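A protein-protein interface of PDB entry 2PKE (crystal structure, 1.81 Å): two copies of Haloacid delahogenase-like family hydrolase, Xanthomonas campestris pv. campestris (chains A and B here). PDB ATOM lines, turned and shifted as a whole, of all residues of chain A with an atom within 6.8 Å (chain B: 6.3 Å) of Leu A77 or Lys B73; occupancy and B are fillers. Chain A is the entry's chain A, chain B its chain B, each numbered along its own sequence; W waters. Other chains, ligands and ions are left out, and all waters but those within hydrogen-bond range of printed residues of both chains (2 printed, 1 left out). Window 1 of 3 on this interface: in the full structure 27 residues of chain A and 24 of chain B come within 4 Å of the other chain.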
ATOM      1  N   VAL A  60     -10.526  13.204 -15.730  1.00  0.00           N
ATOM      2  CA  VAL A  60      -9.502  14.007 -15.076  1.00  0.00           C
ATOM      3  C   VAL A  60      -8.733  14.895 -16.038  1.00  0.00           C
ATOM      4  O   VAL A  60      -8.505  16.065 -15.759  1.00  0.00           O
ATOM      5  CB  VAL A  60      -8.502  13.091 -14.319  1.00  0.00           C
ATOM      6  CG1 VAL A  60      -7.335  13.878 -13.736  1.00  0.00           C
ATOM      7  CG2 VAL A  60      -9.233  12.337 -13.209  1.00  0.00           C
ATOM      8  N   ASN A  64      -8.476  18.995 -15.970  1.00  0.00           N
ATOM      9  CA  ASN A  64      -7.139  19.543 -15.723  1.00  0.00           C
ATOM     10  C   ASN A  64      -6.533  20.309 -16.886  1.00  0.00           C
ATOM     11  O   ASN A  64      -5.592  21.067 -16.701  1.00  0.00           O
ATOM     12  CB  ASN A  64      -6.200  18.442 -15.303  1.00  0.00           C
ATOM     13  CG  ASN A  64      -6.497  17.936 -13.927  1.00  0.00           C
ATOM     14  OD1 ASN A  64      -7.327  18.509 -13.226  1.00  0.00           O
ATOM     15  ND2 ASN A  64      -5.813  16.856 -13.515  1.00  0.00           N
ATOM     16  N   ILE A  67      -6.189  23.945 -16.217  1.00  0.00           N
ATOM     17  CA  ILE A  67      -5.095  24.499 -15.412  1.00  0.00           C
ATOM     18  C   ILE A  67      -3.690  24.144 -15.907  1.00  0.00           C
ATOM     19  O   ILE A  67      -2.734  24.907 -15.676  1.00  0.00           O
ATOM     20  CB  ILE A  67      -5.231  24.178 -13.878  1.00  0.00           C
ATOM     21  CG1 ILE A  67      -5.130  22.701 -13.560  1.00  0.00           C
ATOM     22  CG2 ILE A  67      -6.575  24.653 -13.322  1.00  0.00           C
ATOM     23  CD1 ILE A  67      -4.957  22.455 -12.074  1.00  0.00           C
ATOM     24  N   PHE A  68      -3.549  23.014 -16.598  1.00  0.00           N
ATOM     25  CA  PHE A  68      -2.222  22.571 -17.059  1.00  0.00           C
ATOM     26  C   PHE A  68      -1.933  22.953 -18.488  1.00  0.00           C
ATOM     27  O   PHE A  68      -0.753  23.047 -18.862  1.00  0.00           O
ATOM     28  CB  PHE A  68      -2.097  21.047 -16.974  1.00  0.00           C
ATOM     29  CG  PHE A  68      -2.257  20.499 -15.584  1.00  0.00           C
ATOM     30  CD1 PHE A  68      -1.949  21.230 -14.478  1.00  0.00           C
ATOM     31  CD2 PHE A  68      -2.706  19.198 -15.401  1.00  0.00           C
ATOM     32  CE1 PHE A  68      -2.088  20.677 -13.217  1.00  0.00           C
ATOM     33  CE2 PHE A  68      -2.844  18.667 -14.139  1.00  0.00           C
ATOM     34  CZ  PHE A  68      -2.552  19.413 -13.064  1.00  0.00           C
ATOM     35  N   GLY A  69      -3.006  23.121 -19.287  1.00  0.00           N
ATOM     36  CA  GLY A  69      -2.896  23.050 -20.744  1.00  0.00           C
ATOM     37  C   GLY A  69      -2.370  21.680 -21.217  1.00  0.00           C
ATOM     38  O   GLY A  69      -2.410  20.694 -20.478  1.00  0.00           O
ATOM     39  N   TYR A  70      -1.870  21.627 -22.441  1.00  0.00           N
ATOM     40  CA  TYR A  70      -1.423  20.375 -23.057  1.00  0.00           C
ATOM     41  C   TYR A  70       0.024  20.050 -22.664  1.00  0.00           C
ATOM     42  O   TYR A  70       0.792  20.934 -22.364  1.00  0.00           O
ATOM     43  CB  TYR A  70      -1.503  20.452 -24.573  1.00  0.00           C
ATOM     44  CG  TYR A  70      -2.867  20.711 -25.075  1.00  0.00           C
ATOM     45  CD1 TYR A  70      -3.799  19.678 -25.183  1.00  0.00           C
ATOM     46  CD2 TYR A  70      -3.262  21.984 -25.392  1.00  0.00           C
ATOM     47  CE1 TYR A  70      -5.085  19.927 -25.601  1.00  0.00           C
ATOM     48  CE2 TYR A  70      -4.575  22.242 -25.808  1.00  0.00           C
ATOM     49  CZ  TYR A  70      -5.466  21.206 -25.930  1.00  0.00           C
ATOM     50  OH  TYR A  70      -6.768  21.447 -26.370  1.00  0.00           O
ATOM     51  N   GLY A  71       0.358  18.772 -22.682  1.00  0.00           N
ATOM     52  CA  GLY A  71       1.737  18.311 -22.534  1.00  0.00           C
ATOM     53  C   GLY A  71       1.933  17.223 -21.507  1.00  0.00           C
ATOM     54  O   GLY A  71       1.038  16.916 -20.719  1.00  0.00           O
ATOM     55  N   ALA A  72       3.131  16.642 -21.507  1.00  0.00           N
ATOM     56  CA  ALA A  72       3.462  15.477 -20.638  1.00  0.00           C
ATOM     57  C   ALA A  72       3.456  15.765 -19.149  1.00  0.00           C
ATOM     58  O   ALA A  72       3.177  14.896 -18.342  1.00  0.00           O
ATOM     59  CB  ALA A  72       4.824  14.925 -21.032  1.00  0.00           C
ATOM     60  N   LYS A  73       3.794  16.977 -18.750  1.00  0.00           N
ATOM     61  CA  LYS A  73       3.827  17.290 -17.326  1.00  0.00           C
ATOM     62  C   LYS A  73       2.442  17.221 -16.671  1.00  0.00           C
ATOM     63  O   LYS A  73       2.271  16.589 -15.609  1.00  0.00           O
ATOM     64  CB  LYS A  73       4.524  18.634 -17.110  1.00  0.00           C
ATOM     65  CG  LYS A  73       5.479  18.620 -15.943  1.00  0.00           C
ATOM     66  CD  LYS A  73       6.756  19.405 -16.190  1.00  0.00           C
ATOM     67  CE  LYS A  73       6.538  20.769 -16.721  1.00  0.00           C
ATOM     68  NZ  LYS A  73       7.881  21.396 -16.834  1.00  0.00           N
ATOM     69  N   GLY A  74       1.454  17.826 -17.317  1.00  0.00           N
ATOM     70  CA  GLY A  74       0.073  17.767 -16.865  1.00  0.00           C
ATOM     71  C   GLY A  74      -0.464  16.362 -16.991  1.00  0.00           C
ATOM     72  O   GLY A  74      -1.240  15.917 -16.158  1.00  0.00           O
ATOM     73  N   MET A  75      -0.044  15.660 -18.036  1.00  0.00           N
ATOM     74  CA  MET A  75      -0.444  14.270 -18.232  1.00  0.00           C
ATOM     75  C   MET A  75      -0.072  13.419 -16.994  1.00  0.00           C
ATOM     76  O   MET A  75      -0.900  12.611 -16.525  1.00  0.00           O
ATOM     77  CB  MET A  75       0.262  13.675 -19.442  1.00  0.00           C
ATOM     78  CG  MET A  75      -0.198  12.242 -19.849  1.00  0.00           C
ATOM     79  SD  MET A  75       1.170  11.223 -20.706  1.00  0.00           S
ATOM     80  CE  MET A  75       2.709  11.281 -19.519  1.00  0.00           C
ATOM     81  N   THR A  76       1.161  13.589 -16.506  1.00  0.00           N
ATOM     82  CA  THR A  76       1.647  12.857 -15.322  1.00  0.00           C
ATOM     83  C   THR A  76       0.857  13.118 -14.056  1.00  0.00           C
ATOM     84  O   THR A  76       0.482  12.175 -13.340  1.00  0.00           O
ATOM     85  CB  THR A  76       3.078  13.158 -15.059  1.00  0.00           C
ATOM     86  OG1 THR A  76       3.813  12.824 -16.248  1.00  0.00           O
ATOM     87  CG2 THR A  76       3.600  12.328 -13.887  1.00  0.00           C
ATOM     88  N   LEU A  77       0.575  14.387 -13.811  1.00  0.00           N
ATOM     89  CA  LEU A  77      -0.246  14.801 -12.671  1.00  0.00           C
ATOM     90  C   LEU A  77      -1.694  14.297 -12.784  1.00  0.00           C
ATOM     91  O   LEU A  77      -2.284  13.878 -11.778  1.00  0.00           O
ATOM     92  CB  LEU A  77      -0.230  16.311 -12.525  1.00  0.00           C
ATOM     93  CG  LEU A  77       1.109  16.872 -12.053  1.00  0.00           C
ATOM     94  CD1 LEU A  77       1.067  18.369 -12.341  1.00  0.00           C
ATOM     95  CD2 LEU A  77       1.452  16.554 -10.549  1.00  0.00           C
ATOM     96  N   SER A  78      -2.245  14.300 -13.992  1.00  0.00           N
ATOM     97  CA  SER A  78      -3.590  13.721 -14.188  1.00  0.00           C
ATOM     98  C   SER A  78      -3.572  12.189 -13.968  1.00  0.00           C
ATOM     99  O   SER A  78      -4.511  11.631 -13.451  1.00  0.00           O
ATOM    100  CB  SER A  78      -4.117  14.074 -15.553  1.00  0.00           C
ATOM    101  OG  SER A  78      -4.307  15.494 -15.695  1.00  0.00           O
ATOM    102  N   MET A  79      -2.502  11.517 -14.382  1.00  0.00           N
ATOM    103  CA  MET A  79      -2.343  10.079 -14.137  1.00  0.00           C
ATOM    104  C   MET A  79      -2.243   9.792 -12.673  1.00  0.00           C
ATOM    105  O   MET A  79      -2.727   8.784 -12.240  1.00  0.00           O
ATOM    106  CB  MET A  79      -1.100   9.516 -14.822  1.00  0.00           C
ATOM    107  CG  MET A  79      -1.248   9.365 -16.323  1.00  0.00           C
ATOM    108  SD  MET A  79       0.345   8.563 -17.071  1.00  0.00           S
ATOM    109  CE  MET A  79      -0.515   8.069 -18.751  1.00  0.00           C
ATOM    110  N   ILE A  80      -1.557  10.623 -11.908  1.00  0.00           N
ATOM    111  CA  ILE A  80      -1.388  10.360 -10.471  1.00  0.00           C
ATOM    112  C   ILE A  80      -2.789  10.430  -9.837  1.00  0.00           C
ATOM    113  O   ILE A  80      -3.236   9.522  -9.082  1.00  0.00           O
ATOM    114  CB  ILE A  80      -0.369  11.344  -9.777  1.00  0.00           C
ATOM    115  CG1 ILE A  80       1.092  10.985 -10.159  1.00  0.00           C
ATOM    116  CG2 ILE A  80      -0.552  11.313  -8.242  1.00  0.00           C
ATOM    117  CD1 ILE A  80       2.115  12.151 -10.093  1.00  0.00           C
ATOM    118  N   GLU A  81      -3.482  11.506 -10.178  1.00  0.00           N
ATOM    119  CA  GLU A  81      -4.813  11.779  -9.655  1.00  0.00           C
ATOM    120  C   GLU A  81      -5.784  10.663 -10.024  1.00  0.00           C
ATOM    121  O   GLU A  81      -6.558  10.186  -9.200  1.00  0.00           O
ATOM    122  CB  GLU A  81      -5.232  13.147 -10.183  1.00  0.00           C
ATOM    123  CG  GLU A  81      -6.273  13.864  -9.400  1.00  0.00           C
ATOM    124  CD  GLU A  81      -6.172  15.381  -9.572  1.00  0.00           C
ATOM    125  OE1 GLU A  81      -6.118  15.865 -10.730  1.00  0.00           O
ATOM    126  OE2 GLU A  81      -6.140  16.087  -8.541  1.00  0.00           O
ATOM    127  N   THR A  82      -5.725  10.219 -11.267  1.00  0.00           N
ATOM    128  CA  THR A  82      -6.563   9.107 -11.733  1.00  0.00           C
ATOM    129  C   THR A  82      -6.289   7.783 -11.009  1.00  0.00           C
ATOM    130  O   THR A  82      -7.235   7.041 -10.669  1.00  0.00           O
ATOM    131  CB  THR A  82      -6.345   8.849 -13.217  1.00  0.00           C
ATOM    132  OG1 THR A  82      -6.539  10.055 -13.974  1.00  0.00           O
ATOM    133  CG2 THR A  82      -7.317   7.808 -13.723  1.00  0.00           C
ATOM    134  N   ILE A  99       4.711   6.145 -11.814  1.00  0.00           N
ATOM    135  CA  ILE A  99       3.959   7.039 -12.690  1.00  0.00           C
ATOM    136  C   ILE A  99       4.785   8.303 -12.968  1.00  0.00           C
ATOM    137  O   ILE A  99       4.857   8.758 -14.123  1.00  0.00           O
ATOM    138  CB  ILE A  99       2.629   7.405 -12.087  1.00  0.00           C
ATOM    139  CG1 ILE A  99       1.721   6.156 -12.035  1.00  0.00           C
ATOM    140  CG2 ILE A  99       1.957   8.545 -12.882  1.00  0.00           C
ATOM    141  CD1 ILE A  99       0.456   6.376 -11.300  1.00  0.00           C
ATOM    142  N   ASP A 137       3.718  22.506 -24.355  1.00  0.00           N
ATOM    143  CA  ASP A 137       4.797  22.890 -23.436  1.00  0.00           C
ATOM    144  C   ASP A 137       5.919  23.513 -24.248  1.00  0.00           C
ATOM    145  O   ASP A 137       6.553  22.867 -25.103  1.00  0.00           O
ATOM    146  CB  ASP A 137       5.218  21.633 -22.648  1.00  0.00           C
ATOM    147  CG  ASP A 137       6.320  21.886 -21.607  1.00  0.00           C
ATOM    148  OD1 ASP A 137       7.307  22.600 -21.904  1.00  0.00           O
ATOM    149  OD2 ASP A 137       6.200  21.334 -20.485  1.00  0.00           O
ATOM    150  N   PHE B  68      12.182  18.542 -13.257  1.00  0.00           N
ATOM    151  CA  PHE B  68      10.763  18.751 -13.665  1.00  0.00           C
ATOM    152  C   PHE B  68      10.349  20.188 -13.960  1.00  0.00           C
ATOM    153  O   PHE B  68       9.358  20.418 -14.668  1.00  0.00           O
ATOM    154  CB  PHE B  68       9.843  18.258 -12.582  1.00  0.00           C
ATOM    155  CG  PHE B  68       9.889  16.806 -12.395  1.00  0.00           C
ATOM    156  CD1 PHE B  68       9.435  15.970 -13.388  1.00  0.00           C
ATOM    157  CD2 PHE B  68      10.425  16.273 -11.252  1.00  0.00           C
ATOM    158  CE1 PHE B  68       9.478  14.607 -13.229  1.00  0.00           C
ATOM    159  CE2 PHE B  68      10.478  14.899 -11.071  1.00  0.00           C
ATOM    160  CZ  PHE B  68      10.008  14.058 -12.067  1.00  0.00           C
ATOM    161  N   GLY B  69      11.050  21.146 -13.339  1.00  0.00           N
ATOM    162  CA  GLY B  69      10.759  22.569 -13.549  1.00  0.00           C
ATOM    163  C   GLY B  69      10.467  23.336 -12.287  1.00  0.00           C
ATOM    164  O   GLY B  69      10.178  22.758 -11.243  1.00  0.00           O
ATOM    165  N   TYR B  70      10.545  24.659 -12.414  1.00  0.00           N
ATOM    166  CA  TYR B  70      10.406  25.586 -11.287  1.00  0.00           C
ATOM    167  C   TYR B  70       9.020  26.249 -11.202  1.00  0.00           C
ATOM    168  O   TYR B  70       8.741  27.009 -10.261  1.00  0.00           O
ATOM    169  CB  TYR B  70      11.519  26.636 -11.367  1.00  0.00           C
ATOM    170  CG  TYR B  70      12.878  26.034 -11.053  1.00  0.00           C
ATOM    171  CD1 TYR B  70      13.667  25.477 -12.052  1.00  0.00           C
ATOM    172  CD2 TYR B  70      13.338  25.976  -9.742  1.00  0.00           C
ATOM    173  CE1 TYR B  70      14.895  24.909 -11.763  1.00  0.00           C
ATOM    174  CE2 TYR B  70      14.563  25.417  -9.435  1.00  0.00           C
ATOM    175  CZ  TYR B  70      15.338  24.886 -10.442  1.00  0.00           C
ATOM    176  OH  TYR B  70      16.557  24.329 -10.117  1.00  0.00           O
ATOM    177  N   GLY B  71       8.158  25.934 -12.178  1.00  0.00           N
ATOM    178  CA  GLY B  71       6.774  26.379 -12.195  1.00  0.00           C
ATOM    179  C   GLY B  71       5.945  25.461 -11.348  1.00  0.00           C
ATOM    180  O   GLY B  71       6.466  24.517 -10.735  1.00  0.00           O
ATOM    181  N   ALA B  72       4.648  25.728 -11.284  1.00  0.00           N
ATOM    182  CA  ALA B  72       3.795  24.994 -10.337  1.00  0.00           C
ATOM    183  C   ALA B  72       3.677  23.487 -10.662  1.00  0.00           C
ATOM    184  O   ALA B  72       3.583  22.651  -9.764  1.00  0.00           O
ATOM    185  CB  ALA B  72       2.438  25.617 -10.284  1.00  0.00           C
ATOM    186  N   LYS B  73       3.635  23.129 -11.945  1.00  0.00           N
ATOM    187  CA  LYS B  73       3.595  21.724 -12.307  1.00  0.00           C
ATOM    188  C   LYS B  73       4.877  21.022 -11.904  1.00  0.00           C
ATOM    189  O   LYS B  73       4.853  19.906 -11.347  1.00  0.00           O
ATOM    190  CB  LYS B  73       3.359  21.572 -13.807  1.00  0.00           C
ATOM    191  CG  LYS B  73       1.931  21.776 -14.202  1.00  0.00           C
ATOM    192  CD  LYS B  73       1.778  21.650 -15.733  1.00  0.00           C
ATOM    193  CE  LYS B  73       2.110  22.953 -16.432  1.00  0.00           C
ATOM    194  NZ  LYS B  73       2.075  22.791 -17.908  1.00  0.00           N
ATOM    195  N   GLY B  74       6.012  21.647 -12.216  1.00  0.00           N
ATOM    196  CA  GLY B  74       7.308  21.067 -11.820  1.00  0.00           C
ATOM    197  C   GLY B  74       7.480  21.018 -10.320  1.00  0.00           C
ATOM    198  O   GLY B  74       8.030  20.054  -9.750  1.00  0.00           O
ATOM    199  N   MET B  75       6.971  22.039  -9.660  1.00  0.00           N
ATOM    200  CA  MET B  75       7.047  22.070  -8.202  1.00  0.00           C
ATOM    201  C   MET B  75       6.279  20.869  -7.595  1.00  0.00           C
ATOM    202  O   MET B  75       6.764  20.211  -6.719  1.00  0.00           O
ATOM    203  CB  MET B  75       6.521  23.397  -7.687  1.00  0.00           C
ATOM    204  CG  MET B  75       6.361  23.448  -6.158  1.00  0.00           C
ATOM    205  SD  MET B  75       5.085  24.760  -5.622  1.00  0.00           S
ATOM    206  CE  MET B  75       3.317  24.087  -6.179  1.00  0.00           C
ATOM    207  N   THR B  76       5.111  20.571  -8.126  1.00  0.00           N
ATOM    208  CA  THR B  76       4.256  19.508  -7.612  1.00  0.00           C
ATOM    209  C   THR B  76       4.864  18.129  -7.814  1.00  0.00           C
ATOM    210  O   THR B  76       4.786  17.250  -6.923  1.00  0.00           O
ATOM    211  CB  THR B  76       2.881  19.597  -8.297  1.00  0.00           C
ATOM    212  OG1 THR B  76       2.388  20.925  -8.149  1.00  0.00           O
ATOM    213  CG2 THR B  76       1.848  18.613  -7.722  1.00  0.00           C
ATOM    214  N   LEU B  77       5.415  17.882  -9.004  1.00  0.00           N
ATOM    215  CA  LEU B  77       6.067  16.593  -9.283  1.00  0.00           C
ATOM    216  C   LEU B  77       7.272  16.469  -8.421  1.00  0.00           C
ATOM    217  O   LEU B  77       7.534  15.403  -7.895  1.00  0.00           O
ATOM    218  CB  LEU B  77       6.458  16.479 -10.750  1.00  0.00           C
ATOM    219  CG  LEU B  77       5.279  16.376 -11.705  1.00  0.00           C
ATOM    220  CD1 LEU B  77       5.743  16.713 -13.170  1.00  0.00           C
ATOM    221  CD2 LEU B  77       4.660  15.012 -11.645  1.00  0.00           C
ATOM    222  N   SER B  78       8.021  17.569  -8.263  1.00  0.00           N
ATOM    223  CA  SER B  78       9.197  17.556  -7.388  1.00  0.00           C
ATOM    224  C   SER B  78       8.822  17.322  -5.953  1.00  0.00           C
ATOM    225  O   SER B  78       9.494  16.565  -5.244  1.00  0.00           O
ATOM    226  CB  SER B  78       9.941  18.907  -7.464  1.00  0.00           C
ATOM    227  OG  SER B  78      10.411  19.140  -8.790  1.00  0.00           O
ATOM    228  N   ILE B  80       6.242  15.780  -4.906  1.00  0.00           N
ATOM    229  CA  ILE B  80       5.850  14.373  -4.858  1.00  0.00           C
ATOM    230  C   ILE B  80       7.027  13.412  -4.777  1.00  0.00           C
ATOM    231  O   ILE B  80       7.035  12.511  -3.920  1.00  0.00           O
ATOM    232  CB  ILE B  80       4.906  13.999  -6.049  1.00  0.00           C
ATOM    233  CG1 ILE B  80       3.489  14.598  -5.833  1.00  0.00           C
ATOM    234  CG2 ILE B  80       4.770  12.505  -6.153  1.00  0.00           C
ATOM    235  CD1 ILE B  80       2.596  14.610  -7.086  1.00  0.00           C
ATOM    236  N   VAL B 100      -0.866  17.151  -4.724  1.00  0.00           N
ATOM    237  CA  VAL B 100      -1.434  17.526  -6.004  1.00  0.00           C
ATOM    238  C   VAL B 100      -2.344  18.723  -5.777  1.00  0.00           C
ATOM    239  O   VAL B 100      -2.246  19.675  -6.510  1.00  0.00           O
ATOM    240  CB  VAL B 100      -2.166  16.361  -6.685  1.00  0.00           C
ATOM    241  CG1 VAL B 100      -2.848  16.827  -7.969  1.00  0.00           C
ATOM    242  CG2 VAL B 100      -1.173  15.198  -6.982  1.00  0.00           C
ATOM    243  N   GLY B 103      -0.470  22.036  -5.742  1.00  0.00           N
ATOM    244  CA  GLY B 103      -0.082  22.520  -7.058  1.00  0.00           C
ATOM    245  C   GLY B 103      -1.287  23.100  -7.768  1.00  0.00           C
ATOM    246  O   GLY B 103      -1.194  24.146  -8.417  1.00  0.00           O
ATOM    247  N   LEU B 107      -1.660  26.791  -9.052  1.00  0.00           N
ATOM    248  CA  LEU B 107      -1.979  27.104 -10.435  1.00  0.00           C
ATOM    249  C   LEU B 107      -3.213  27.985 -10.610  1.00  0.00           C
ATOM    250  O   LEU B 107      -3.347  28.668 -11.630  1.00  0.00           O
ATOM    251  CB  LEU B 107      -2.179  25.811 -11.232  1.00  0.00           C
ATOM    252  CG  LEU B 107      -0.896  25.121 -11.687  1.00  0.00           C
ATOM    253  CD1 LEU B 107      -1.191  23.711 -12.054  1.00  0.00           C
ATOM    254  CD2 LEU B 107      -0.225  25.873 -12.847  1.00  0.00           C
ATOM    255  N   ASP B 137       6.278  28.487 -17.547  1.00  0.00           N
ATOM    256  CA  ASP B 137       5.311  27.672 -18.211  1.00  0.00           C
ATOM    257  C   ASP B 137       4.395  28.534 -19.040  1.00  0.00           C
ATOM    258  O   ASP B 137       3.760  29.490 -18.551  1.00  0.00           O
ATOM    259  CB  ASP B 137       4.504  26.890 -17.173  1.00  0.00           C
ATOM    260  CG  ASP B 137       3.484  25.928 -17.804  1.00  0.00           C
ATOM    261  OD1 ASP B 137       3.891  24.860 -18.273  1.00  0.00           O
ATOM    262  OD2 ASP B 137       2.260  26.215 -17.772  1.00  0.00           O
ATOM    263  N   PHE B 139       1.472  28.023 -20.478  1.00  0.00           N
ATOM    264  CA  PHE B 139       0.069  28.079 -20.139  1.00  0.00           C
ATOM    265  C   PHE B 139      -0.176  28.954 -18.910  1.00  0.00           C
ATOM    266  O   PHE B 139      -1.071  29.817 -18.932  1.00  0.00           O
ATOM    267  CB  PHE B 139      -0.500  26.656 -19.910  1.00  0.00           C
ATOM    268  CG  PHE B 139      -1.976  26.630 -19.726  1.00  0.00           C
ATOM    269  CD1 PHE B 139      -2.808  26.579 -20.823  1.00  0.00           C
ATOM    270  CD2 PHE B 139      -2.540  26.681 -18.467  1.00  0.00           C
ATOM    271  CE1 PHE B 139      -4.192  26.561 -20.680  1.00  0.00           C
ATOM    272  CE2 PHE B 139      -3.932  26.683 -18.319  1.00  0.00           C
ATOM    273  CZ  PHE B 139      -4.741  26.627 -19.441  1.00  0.00           C
ATOM    274  N   HIS B 140       0.589  28.733 -17.845  1.00  0.00           N
ATOM    275  CA  HIS B 140       0.339  29.420 -16.573  1.00  0.00           C
ATOM    276  C   HIS B 140       0.699  30.907 -16.720  1.00  0.00           C
ATOM    277  O   HIS B 140      -0.033  31.780 -16.234  1.00  0.00           O
ATOM    278  CB  HIS B 140       1.097  28.743 -15.450  1.00  0.00           C
ATOM    279  CG  HIS B 140       0.773  29.240 -14.082  1.00  0.00           C
ATOM    280  ND1 HIS B 140       1.616  29.022 -13.024  1.00  0.00           N
ATOM    281  CD2 HIS B 140      -0.292  29.909 -13.584  1.00  0.00           C
ATOM    282  CE1 HIS B 140       1.101  29.554 -11.928  1.00  0.00           C
ATOM    283  NE2 HIS B 140      -0.074  30.074 -12.236  1.00  0.00           N
HETATM  284  O   HOH W   1       6.427  24.005 -17.894  1.00  0.00           O
HETATM  285  O   HOH W   2       0.877  23.125 -21.142  1.00  0.00           O
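The side-chain amino group of Lys B73 sits at hydrogen-bond distance from the backbone carbonyl oxygen of Phe A68, 3.0 Å away. The side-chain amino group of Lys A73 lies within hydrogen-bond range of the backbone carbonyl oxygen of Phe B68.
The side-chain amide nitrogen (ND2) of Asn A64 is in hydrogen-bond range of the side-chain carboxylate (OE1) of Glu A81. The backbone carbonyl oxygen (O) of Ala A72 sits at hydrogen-bond distance from the side-chain hydroxyl (OG1) of Thr A76, at 3.0 Å. The backbone carbonyl oxygen of Ala B72 is in hydrogen-bond range of the side-chain hydroxyl of Thr B76, 2.6 Å away. The side-chain amino group (NZ) of Lys B73 is in salt-bridge range of the side-chain carboxylate (OD1) of Asp B137 (2.8 Å). The side-chain carboxylate (OD2) of Asp B137 sits close to the backbone NH (N) of Phe B139, at 3.3 Å.
Ile A67 touches Leu B107 (O to CD2, 3.9 Å). O of Ile A67 touches CD2 of Phe B139, at 3.3 Å. Leu B107 touches Phe A68 (CD1 to CE1, 3.4 Å). CB of Phe B139 touches O of Phe A68, 3.8 Å away. Lys A73 touches Leu B77 (CG to CD1, 3.4 Å). Thr A76 touches Leu B77. Leu A77 touches Lys B73. Leu B77 touches Leu A77. Ile A80 touches Ile B80. Val B100 touches Glu A81.
Of the printed residues of chain B, Ile A67 touches Leu B107 and Phe B139. Of the printed residues of chain B, Leu A77 touches Lys B73, Thr B76 and Leu B77. Of the printed residues of chain B, Glu A81 touches Val B100 (3.4 Å). Printed residues of chain A within 4 Å of Phe B68: Lys A73 (2.8 Å). Lys B73 touches just these residues of chain A: Phe A68 and Leu A77. Of the printed residues of chain A, Leu B107 touches Ile A67 (3.9 Å) and Phe A68 (3.4 Å). Asp B137 touches none of the printed residues of chain A. Printed residues of chain A within 4 Å of Phe B139: Ile A67, Phe A68 and Gly A69. His B140 touches none of the printed residues of chain A. The nearest residue of chain B that does not touch Leu A77 is Ile B80 (4.1 Å).
Of the 18 printed residues of chain B, 8 touch a printed residue of chain A. Printed residues of chain A that touch a printed residue of chain B: Ile A67, Phe A68, Gly A69, Lys A73, Thr A76, Leu A77, Ile A80 and Glu A81. Hydrophobic or aromatic side chains of chain A that line the printed part of chain B: Ile A67, Phe A68, Leu A77 and Ile A80. Along chain A the printed residues that touch a printed residue of chain B span positions 67 to 81. Among the printed residues, no Asp or Glu carboxylate lies within 4 Å of a Lys or Arg side-chain nitrogen of the other chain.
Phe A68 touches Lys B73, and with the chains exchanged Lys A73 touches Phe B68. Thr A76 touches Leu B77, and with the chains exchanged Leu A77 touches Thr B76. Leu A77 touches its own counterpart, Leu B77. Ile B80 touches its own counterpart, Ile A80. 13 positions are printed for both chains.
Water W2 lies within hydrogen-bond range of O of Tyr A70, O of Phe A68 and NZ of Lys B73. Water W1 bridges the side-chain carboxylate (OD1) of Asp B137 (2.7 Å) and the side-chain amino group (NZ) of Lys A73 (3.2 Å).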
